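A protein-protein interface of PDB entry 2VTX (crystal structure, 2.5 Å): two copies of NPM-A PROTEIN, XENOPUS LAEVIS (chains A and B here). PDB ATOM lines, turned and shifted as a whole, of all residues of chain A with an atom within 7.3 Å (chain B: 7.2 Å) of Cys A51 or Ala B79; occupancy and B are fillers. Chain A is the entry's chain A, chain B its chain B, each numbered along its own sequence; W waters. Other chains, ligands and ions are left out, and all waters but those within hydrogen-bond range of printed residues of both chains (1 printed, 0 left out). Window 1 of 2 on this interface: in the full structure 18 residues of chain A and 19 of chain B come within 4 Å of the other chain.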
ATOM      1  N   CYS A  21      11.178 -22.036 -24.687  1.00  0.00           N
ATOM      2  CA  CYS A  21      12.174 -22.567 -23.780  1.00  0.00           C
ATOM      3  C   CYS A  21      11.635 -22.694 -22.385  1.00  0.00           C
ATOM      4  O   CYS A  21      10.610 -22.097 -22.102  1.00  0.00           O
ATOM      5  CB  CYS A  21      13.428 -21.732 -23.773  1.00  0.00           C
ATOM      6  SG  CYS A  21      13.309 -20.165 -23.054  1.00  0.00           S
ATOM      7  N   LEU A  23      12.641 -22.221 -18.433  1.00  0.00           N
ATOM      8  CA  LEU A  23      13.597 -21.814 -17.427  1.00  0.00           C
ATOM      9  C   LEU A  23      13.130 -22.471 -16.135  1.00  0.00           C
ATOM     10  O   LEU A  23      11.982 -22.668 -15.918  1.00  0.00           O
ATOM     11  CB  LEU A  23      13.689 -20.335 -17.278  1.00  0.00           C
ATOM     12  CG  LEU A  23      13.865 -19.476 -18.470  1.00  0.00           C
ATOM     13  CD1 LEU A  23      13.679 -18.027 -18.060  1.00  0.00           C
ATOM     14  CD2 LEU A  23      15.166 -19.724 -19.122  1.00  0.00           C
ATOM     15  N   THR A  49       4.268 -15.231 -25.285  1.00  0.00           N
ATOM     16  CA  THR A  49       3.689 -15.444 -23.971  1.00  0.00           C
ATOM     17  C   THR A  49       4.797 -15.963 -23.021  1.00  0.00           C
ATOM     18  O   THR A  49       5.802 -16.456 -23.525  1.00  0.00           O
ATOM     19  CB  THR A  49       2.520 -16.528 -24.030  1.00  0.00           C
ATOM     20  OG1 THR A  49       3.087 -17.842 -24.258  1.00  0.00           O
ATOM     21  CG2 THR A  49       1.534 -16.187 -25.107  1.00  0.00           C
ATOM     22  N   VAL A  50       4.559 -15.853 -21.694  1.00  0.00           N
ATOM     23  CA  VAL A  50       5.331 -16.427 -20.657  1.00  0.00           C
ATOM     24  C   VAL A  50       4.307 -17.107 -19.785  1.00  0.00           C
ATOM     25  O   VAL A  50       3.310 -16.569 -19.568  1.00  0.00           O
ATOM     26  CB  VAL A  50       6.070 -15.356 -19.819  1.00  0.00           C
ATOM     27  CG1 VAL A  50       6.744 -16.042 -18.678  1.00  0.00           C
ATOM     28  CG2 VAL A  50       7.323 -14.767 -20.599  1.00  0.00           C
ATOM     29  N   CYS A  51       4.589 -18.276 -19.255  1.00  0.00           N
ATOM     30  CA  CYS A  51       3.673 -18.952 -18.461  1.00  0.00           C
ATOM     31  C   CYS A  51       4.284 -19.974 -17.549  1.00  0.00           C
ATOM     32  O   CYS A  51       5.342 -20.455 -17.775  1.00  0.00           O
ATOM     33  CB  CYS A  51       2.656 -19.550 -19.356  1.00  0.00           C
ATOM     34  SG  CYS A  51       2.989 -20.884 -20.390  1.00  0.00           S
ATOM     35  N   LEU A  52       3.635 -20.258 -16.437  1.00  0.00           N
ATOM     36  CA  LEU A  52       4.146 -21.187 -15.452  1.00  0.00           C
ATOM     37  C   LEU A  52       3.619 -22.616 -15.676  1.00  0.00           C
ATOM     38  O   LEU A  52       2.496 -22.822 -16.185  1.00  0.00           O
ATOM     39  CB  LEU A  52       3.748 -20.725 -14.078  1.00  0.00           C
ATOM     40  CG  LEU A  52       4.266 -19.388 -13.560  1.00  0.00           C
ATOM     41  CD1 LEU A  52       3.852 -19.101 -12.168  1.00  0.00           C
ATOM     42  CD2 LEU A  52       5.793 -19.268 -13.763  1.00  0.00           C
ATOM     43  N   GLY A  53       4.402 -23.585 -15.206  1.00  0.00           N
ATOM     44  CA  GLY A  53       4.016 -24.932 -15.182  1.00  0.00           C
ATOM     45  C   GLY A  53       3.181 -25.176 -13.991  1.00  0.00           C
ATOM     46  O   GLY A  53       3.203 -24.413 -13.047  1.00  0.00           O
ATOM     47  N   LEU A  81       5.372 -13.336 -12.383  1.00  0.00           N
ATOM     48  CA  LEU A  81       4.253 -14.230 -12.408  1.00  0.00           C
ATOM     49  C   LEU A  81       4.231 -14.920 -11.051  1.00  0.00           C
ATOM     50  O   LEU A  81       5.258 -15.009 -10.322  1.00  0.00           O
ATOM     51  CB  LEU A  81       4.450 -15.306 -13.465  1.00  0.00           C
ATOM     52  CG  LEU A  81       4.468 -14.731 -14.938  1.00  0.00           C
ATOM     53  CD1 LEU A  81       4.797 -15.789 -15.996  1.00  0.00           C
ATOM     54  CD2 LEU A  81       3.147 -13.927 -15.342  1.00  0.00           C
ATOM     55  N   LEU A  86      -1.065 -14.694 -10.891  1.00  0.00           N
ATOM     56  CA  LEU A  86      -1.033 -14.361 -12.313  1.00  0.00           C
ATOM     57  C   LEU A  86      -0.039 -15.364 -12.959  1.00  0.00           C
ATOM     58  O   LEU A  86       1.190 -15.258 -12.805  1.00  0.00           O
ATOM     59  CB  LEU A  86      -0.500 -12.978 -12.541  1.00  0.00           C
ATOM     60  CG  LEU A  86      -0.551 -12.567 -14.032  1.00  0.00           C
ATOM     61  CD1 LEU A  86      -1.983 -12.306 -14.609  1.00  0.00           C
ATOM     62  CD2 LEU A  86       0.330 -11.311 -14.275  1.00  0.00           C
ATOM     63  N   PRO A  87      -0.586 -16.438 -13.492  1.00  0.00           N
ATOM     64  CA  PRO A  87       0.137 -17.469 -13.971  1.00  0.00           C
ATOM     65  C   PRO A  87       0.619 -17.403 -15.391  1.00  0.00           C
ATOM     66  O   PRO A  87       1.295 -18.323 -15.834  1.00  0.00           O
ATOM     67  CB  PRO A  87      -0.824 -18.627 -13.766  1.00  0.00           C
ATOM     68  CG  PRO A  87      -2.160 -18.152 -14.051  1.00  0.00           C
ATOM     69  CD  PRO A  87      -2.027 -16.766 -13.395  1.00  0.00           C
ATOM     70  N   MET A  88       0.289 -16.383 -16.134  1.00  0.00           N
ATOM     71  CA  MET A  88       0.908 -16.225 -17.430  1.00  0.00           C
ATOM     72  C   MET A  88       0.758 -14.737 -17.853  1.00  0.00           C
ATOM     73  O   MET A  88       0.055 -13.982 -17.276  1.00  0.00           O
ATOM     74  CB  MET A  88       0.257 -17.131 -18.446  1.00  0.00           C
ATOM     75  CG  MET A  88      -1.151 -16.619 -18.828  1.00  0.00           C
ATOM     76  SD  MET A  88      -1.893 -17.423 -20.237  1.00  0.00           S
ATOM     77  CE  MET A  88      -1.056 -16.475 -21.465  1.00  0.00           C
ATOM     78  N   ALA A  89       1.420 -14.357 -18.915  1.00  0.00           N
ATOM     79  CA  ALA A  89       1.292 -13.030 -19.487  1.00  0.00           C
ATOM     80  C   ALA A  89       1.613 -13.098 -20.999  1.00  0.00           C
ATOM     81  O   ALA A  89       2.307 -13.987 -21.462  1.00  0.00           O
ATOM     82  CB  ALA A  89       2.182 -12.054 -18.808  1.00  0.00           C
ATOM     83  N   PRO A 110       8.830 -24.718 -13.297  1.00  0.00           N
ATOM     84  CA  PRO A 110       9.065 -24.325 -14.675  1.00  0.00           C
ATOM     85  C   PRO A 110       8.418 -23.055 -15.060  1.00  0.00           C
ATOM     86  O   PRO A 110       7.315 -22.808 -14.657  1.00  0.00           O
ATOM     87  CB  PRO A 110       8.470 -25.468 -15.472  1.00  0.00           C
ATOM     88  CG  PRO A 110       8.353 -26.674 -14.518  1.00  0.00           C
ATOM     89  CD  PRO A 110       8.312 -26.101 -13.125  1.00  0.00           C
ATOM     90  N   LEU A 111       9.135 -22.231 -15.829  1.00  0.00           N
ATOM     91  CA  LEU A 111       8.578 -21.088 -16.457  1.00  0.00           C
ATOM     92  C   LEU A 111       8.800 -21.289 -17.912  1.00  0.00           C
ATOM     93  O   LEU A 111       9.934 -21.621 -18.294  1.00  0.00           O
ATOM     94  CB  LEU A 111       9.324 -19.856 -16.037  1.00  0.00           C
ATOM     95  CG  LEU A 111       8.807 -18.575 -16.620  1.00  0.00           C
ATOM     96  CD1 LEU A 111       8.812 -17.449 -15.557  1.00  0.00           C
ATOM     97  CD2 LEU A 111       9.587 -18.100 -17.913  1.00  0.00           C
ATOM     98  N   TYR A 112       7.792 -21.119 -18.731  1.00  0.00           N
ATOM     99  CA  TYR A 112       7.898 -21.335 -20.135  1.00  0.00           C
ATOM    100  C   TYR A 112       7.798 -20.028 -20.897  1.00  0.00           C
ATOM    101  O   TYR A 112       7.027 -19.179 -20.515  1.00  0.00           O
ATOM    102  CB  TYR A 112       6.757 -22.271 -20.610  1.00  0.00           C
ATOM    103  CG  TYR A 112       6.654 -23.598 -19.898  1.00  0.00           C
ATOM    104  CD1 TYR A 112       5.660 -23.849 -19.062  1.00  0.00           C
ATOM    105  CD2 TYR A 112       7.542 -24.634 -20.174  1.00  0.00           C
ATOM    106  CE1 TYR A 112       5.535 -25.110 -18.421  1.00  0.00           C
ATOM    107  CE2 TYR A 112       7.478 -25.816 -19.532  1.00  0.00           C
ATOM    108  CZ  TYR A 112       6.431 -26.080 -18.679  1.00  0.00           C
ATOM    109  OH  TYR A 112       6.314 -27.340 -18.058  1.00  0.00           O
ATOM    110  N   ILE A 113       8.585 -19.825 -21.950  1.00  0.00           N
ATOM    111  CA  ILE A 113       8.530 -18.675 -22.782  1.00  0.00           C
ATOM    112  C   ILE A 113       8.196 -19.119 -24.180  1.00  0.00           C
ATOM    113  O   ILE A 113       8.791 -20.045 -24.630  1.00  0.00           O
ATOM    114  CB  ILE A 113       9.968 -18.024 -22.884  1.00  0.00           C
ATOM    115  CG1 ILE A 113      10.490 -17.737 -21.485  1.00  0.00           C
ATOM    116  CG2 ILE A 113       9.928 -16.712 -23.723  1.00  0.00           C
ATOM    117  CD1 ILE A 113      11.744 -16.754 -21.404  1.00  0.00           C
ATOM    118  N   SER A 114       7.368 -18.406 -24.947  1.00  0.00           N
ATOM    119  CA  SER A 114       7.141 -18.878 -26.281  1.00  0.00           C
ATOM    120  C   SER A 114       7.478 -17.698 -27.137  1.00  0.00           C
ATOM    121  O   SER A 114       7.372 -16.560 -26.666  1.00  0.00           O
ATOM    122  CB  SER A 114       5.697 -19.337 -26.469  1.00  0.00           C
ATOM    123  OG  SER A 114       4.801 -18.199 -26.258  1.00  0.00           O
ATOM    124  N   VAL B  50      -7.936 -17.713 -25.455  1.00  0.00           N
ATOM    125  CA  VAL B  50      -7.964 -19.045 -24.895  1.00  0.00           C
ATOM    126  C   VAL B  50      -8.803 -18.874 -23.654  1.00  0.00           C
ATOM    127  O   VAL B  50      -8.636 -17.931 -22.916  1.00  0.00           O
ATOM    128  CB  VAL B  50      -6.470 -19.534 -24.565  1.00  0.00           C
ATOM    129  CG1 VAL B  50      -6.497 -20.678 -23.644  1.00  0.00           C
ATOM    130  CG2 VAL B  50      -5.728 -19.967 -25.830  1.00  0.00           C
ATOM    131  N   HIS B  61      -4.523 -25.467 -16.123  1.00  0.00           N
ATOM    132  CA  HIS B  61      -4.787 -25.956 -17.459  1.00  0.00           C
ATOM    133  C   HIS B  61      -3.731 -25.322 -18.298  1.00  0.00           C
ATOM    134  O   HIS B  61      -3.509 -24.130 -18.122  1.00  0.00           O
ATOM    135  CB  HIS B  61      -6.089 -25.447 -17.998  1.00  0.00           C
ATOM    136  CG  HIS B  61      -7.292 -26.106 -17.412  1.00  0.00           C
ATOM    137  ND1 HIS B  61      -7.700 -25.877 -16.125  1.00  0.00           N
ATOM    138  CD2 HIS B  61      -8.231 -26.909 -17.970  1.00  0.00           C
ATOM    139  CE1 HIS B  61      -8.797 -26.584 -15.881  1.00  0.00           C
ATOM    140  NE2 HIS B  61      -9.119 -27.248 -16.972  1.00  0.00           N
ATOM    141  N   ILE B  62      -3.000 -26.114 -19.106  1.00  0.00           N
ATOM    142  CA  ILE B  62      -1.885 -25.650 -19.891  1.00  0.00           C
ATOM    143  C   ILE B  62      -2.024 -26.145 -21.276  1.00  0.00           C
ATOM    144  O   ILE B  62      -2.234 -27.302 -21.481  1.00  0.00           O
ATOM    145  CB  ILE B  62      -0.515 -26.168 -19.357  1.00  0.00           C
ATOM    146  CG1 ILE B  62      -0.307 -25.703 -17.920  1.00  0.00           C
ATOM    147  CG2 ILE B  62       0.649 -25.633 -20.274  1.00  0.00           C
ATOM    148  CD1 ILE B  62       0.980 -26.190 -17.253  1.00  0.00           C
ATOM    149  N   VAL B  63      -1.961 -25.259 -22.236  1.00  0.00           N
ATOM    150  CA  VAL B  63      -2.167 -25.598 -23.630  1.00  0.00           C
ATOM    151  C   VAL B  63      -0.853 -25.368 -24.368  1.00  0.00           C
ATOM    152  O   VAL B  63      -0.238 -24.348 -24.196  1.00  0.00           O
ATOM    153  CB  VAL B  63      -3.328 -24.754 -24.256  1.00  0.00           C
ATOM    154  CG1 VAL B  63      -3.167 -23.353 -23.816  1.00  0.00           C
ATOM    155  CG2 VAL B  63      -3.271 -24.838 -25.784  1.00  0.00           C
ATOM    156  N   GLU B  64      -0.404 -26.383 -25.128  1.00  0.00           N
ATOM    157  CA  GLU B  64       0.844 -26.348 -25.807  1.00  0.00           C
ATOM    158  C   GLU B  64       0.693 -26.545 -27.279  1.00  0.00           C
ATOM    159  O   GLU B  64      -0.240 -27.166 -27.700  1.00  0.00           O
ATOM    160  CB  GLU B  64       1.808 -27.340 -25.160  1.00  0.00           C
ATOM    161  CG  GLU B  64       1.489 -28.865 -25.217  1.00  0.00           C
ATOM    162  CD  GLU B  64       2.438 -29.702 -24.345  1.00  0.00           C
ATOM    163  OE1 GLU B  64       2.200 -30.916 -23.940  1.00  0.00           O
ATOM    164  OE2 GLU B  64       3.485 -29.158 -24.054  1.00  0.00           O
ATOM    165  N   VAL B  76       5.608 -26.436 -27.067  1.00  0.00           N
ATOM    166  CA  VAL B  76       5.844 -25.167 -26.580  1.00  0.00           C
ATOM    167  C   VAL B  76       4.601 -24.800 -25.802  1.00  0.00           C
ATOM    168  O   VAL B  76       3.591 -24.432 -26.369  1.00  0.00           O
ATOM    169  CB  VAL B  76       6.069 -24.256 -27.761  1.00  0.00           C
ATOM    170  CG1 VAL B  76       6.178 -22.838 -27.352  1.00  0.00           C
ATOM    171  CG2 VAL B  76       7.331 -24.693 -28.470  1.00  0.00           C
ATOM    172  N   PRO B  77       4.650 -24.905 -24.467  1.00  0.00           N
ATOM    173  CA  PRO B  77       3.560 -24.207 -23.719  1.00  0.00           C
ATOM    174  C   PRO B  77       3.361 -22.735 -24.094  1.00  0.00           C
ATOM    175  O   PRO B  77       4.347 -22.010 -24.243  1.00  0.00           O
ATOM    176  CB  PRO B  77       3.933 -24.372 -22.289  1.00  0.00           C
ATOM    177  CG  PRO B  77       4.752 -25.658 -22.330  1.00  0.00           C
ATOM    178  CD  PRO B  77       5.534 -25.636 -23.609  1.00  0.00           C
ATOM    179  N   ILE B  78       2.079 -22.348 -24.302  1.00  0.00           N
ATOM    180  CA  ILE B  78       1.691 -20.976 -24.674  1.00  0.00           C
ATOM    181  C   ILE B  78       0.708 -20.300 -23.761  1.00  0.00           C
ATOM    182  O   ILE B  78       0.657 -19.035 -23.827  1.00  0.00           O
ATOM    183  CB  ILE B  78       1.119 -20.897 -26.125  1.00  0.00           C
ATOM    184  CG1 ILE B  78      -0.106 -21.784 -26.316  1.00  0.00           C
ATOM    185  CG2 ILE B  78       2.213 -21.313 -27.085  1.00  0.00           C
ATOM    186  CD1 ILE B  78      -0.909 -21.474 -27.606  1.00  0.00           C
ATOM    187  N   ALA B  79      -0.036 -21.059 -22.915  1.00  0.00           N
ATOM    188  CA  ALA B  79      -0.992 -20.460 -21.976  1.00  0.00           C
ATOM    189  C   ALA B  79      -1.118 -21.295 -20.729  1.00  0.00           C
ATOM    190  O   ALA B  79      -1.113 -22.491 -20.892  1.00  0.00           O
ATOM    191  CB  ALA B  79      -2.402 -20.297 -22.628  1.00  0.00           C
ATOM    192  N   THR B  80      -1.183 -20.692 -19.528  1.00  0.00           N
ATOM    193  CA  THR B  80      -1.569 -21.378 -18.309  1.00  0.00           C
ATOM    194  C   THR B  80      -2.764 -20.680 -17.690  1.00  0.00           C
ATOM    195  O   THR B  80      -2.729 -19.454 -17.502  1.00  0.00           O
ATOM    196  CB  THR B  80      -0.409 -21.446 -17.318  1.00  0.00           C
ATOM    197  OG1 THR B  80       0.647 -22.162 -17.949  1.00  0.00           O
ATOM    198  CG2 THR B  80      -0.771 -22.175 -15.927  1.00  0.00           C
ATOM    199  N   LEU B  81      -3.854 -21.396 -17.509  1.00  0.00           N
ATOM    200  CA  LEU B  81      -5.005 -20.819 -16.908  1.00  0.00           C
ATOM    201  C   LEU B  81      -5.542 -21.580 -15.681  1.00  0.00           C
ATOM    202  O   LEU B  81      -5.207 -22.713 -15.481  1.00  0.00           O
ATOM    203  CB  LEU B  81      -6.091 -20.765 -17.926  1.00  0.00           C
ATOM    204  CG  LEU B  81      -5.805 -20.052 -19.254  1.00  0.00           C
ATOM    205  CD1 LEU B  81      -6.998 -20.376 -20.286  1.00  0.00           C
ATOM    206  CD2 LEU B  81      -5.680 -18.487 -19.125  1.00  0.00           C
ATOM    207  N   ALA B  89      -7.074 -15.816 -21.553  1.00  0.00           N
ATOM    208  CA  ALA B  89      -5.948 -15.008 -21.975  1.00  0.00           C
ATOM    209  C   ALA B  89      -6.155 -14.486 -23.447  1.00  0.00           C
ATOM    210  O   ALA B  89      -6.748 -15.162 -24.297  1.00  0.00           O
ATOM    211  CB  ALA B  89      -4.723 -15.806 -21.828  1.00  0.00           C
ATOM    212  N   MET B  91      -4.505 -13.714 -26.880  1.00  0.00           N
ATOM    213  CA  MET B  91      -3.320 -14.083 -27.639  1.00  0.00           C
ATOM    214  C   MET B  91      -3.090 -13.011 -28.677  1.00  0.00           C
ATOM    215  O   MET B  91      -3.981 -12.606 -29.391  1.00  0.00           O
ATOM    216  CB  MET B  91      -3.564 -15.392 -28.341  1.00  0.00           C
ATOM    217  CG  MET B  91      -3.913 -16.608 -27.387  1.00  0.00           C
ATOM    218  SD  MET B  91      -2.568 -17.313 -26.296  1.00  0.00           S
ATOM    219  CE  MET B  91      -2.976 -16.539 -24.826  1.00  0.00           C
ATOM    220  N   LEU B 111     -11.273 -26.370 -22.381  1.00  0.00           N
ATOM    221  CA  LEU B 111     -10.512 -25.197 -22.676  1.00  0.00           C
ATOM    222  C   LEU B 111     -10.744 -24.830 -24.196  1.00  0.00           C
ATOM    223  O   LEU B 111     -10.634 -25.695 -25.122  1.00  0.00           O
ATOM    224  CB  LEU B 111      -9.076 -25.494 -22.316  1.00  0.00           C
ATOM    225  CG  LEU B 111      -8.082 -24.422 -22.767  1.00  0.00           C
ATOM    226  CD1 LEU B 111      -6.793 -24.582 -21.865  1.00  0.00           C
ATOM    227  CD2 LEU B 111      -7.786 -24.554 -24.210  1.00  0.00           C
HETATM  228  O   HOH W   1       7.038 -22.456 -24.171  1.00  0.00           O
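Cys A51 touches just these residues of chain B: Ala B79 and Thr B80.
Of chain A, only Cys A51 (3.9 Å) and Met A88 (3.6 Å) come within 4 Å of Ala B79.
Of the printed residues of chain B, Leu A52 touches Ile B62 and Thr B80.
Of the printed residues of chain A, Pro B77 touches Tyr A112 (3.7 Å) and Ser A114 (3.7 Å).
Printed residues of chain B within 4 Å of Tyr A112: Pro B77 (3.7 Å).
Of the printed residues of chain B, Pro A87 touches Thr B80.
Of the printed residues of chain A, Ile B62 touches Leu A52 (3.8 Å) and Gly A53 (3.9 Å).
Leu B81 touches none of the printed residues of chain A.
The nearest printed residue of chain B that does not touch Cys A51 is Pro B77 (4.1 Å).
The nearest printed residue of chain B that does not touch Ser A114 is Ile B78 (4.1 Å).
Positions printed for both chains: 50, 81, 89 and 111.
Of the 15 pairs that touch across the chains among the printed residues, none has its exchanged pair printed and touching as well.
The side-chain hydroxyl of Thr A49 sits at hydrogen-bond distance from the backbone carbonyl oxygen of Ile B78, at 2.7 Å.
The side-chain sulfur (SD) of Met A88 lies within hydrogen-bond range of the backbone NH (N) of Thr B80 (3.4 Å).
OG1 of Thr B80 sits close to SG of Cys A51, at 3.6 Å.
OG1 of Thr B80 lies within hydrogen-bond range of O of Leu A52, 2.6 Å away.
Cys A51 touches Ala B79.
CD1 of Ile B62 touches O of Leu A52, at 3.8 Å.
Pro A87 touches Thr B80.
Ile B78 touches Met A88.
Met A88 touches Ala B79 (SD to CA, 3.6 Å).
CB of Ala B89 touches SD of Met A88, 3.6 Å away.
Met B91 touches Met A88 (CE to CE, 3.9 Å).
Pro B77 touches Tyr A112.
Ser A114 touches Val B76.
CB of Ser A114 touches O of Pro B77, at 3.7 Å.
Water W1 lies within hydrogen-bond range of the backbone carbonyl oxygen (O) of Pro B77 (2.7 Å) and the backbone carbonyl oxygen (O) of Ile A113 (3.0 Å).
The backbone carbonyl oxygen (O) of Cys A51 lies within hydrogen-bond range of the backbone NH (N) of Tyr A112 (2.7 Å).
The backbone carbonyl oxygen (O) of Ala B79 sits at hydrogen-bond distance from the backbone NH (N) of Val B63.
The backbone carbonyl oxygen of Pro A110 is in hydrogen-bond range of the backbone NH of Gly A53 (3.1 Å).
OG1 of Thr A49 is in hydrogen-bond range of OG of Ser A114 (2.7 Å).
O of Val B63 sits at hydrogen-bond distance from N of Ile B78 (3.1 Å).
O of Pro A87 sits at hydrogen-bond distance from N of Leu A52 (3.1 Å).
Of the 17 printed residues of chain A, 8 touch a printed residue of chain B.
Printed residues of chain A that touch a printed residue of chain B: Thr A49, Cys A51, Leu A52, Gly A53, Pro A87, Met A88, Tyr A112 and Ser A114.
Along chain B the printed residues that touch a printed residue of chain A span positions 62 to 91.
Among the printed residues, 15 pairs touch across the chains.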
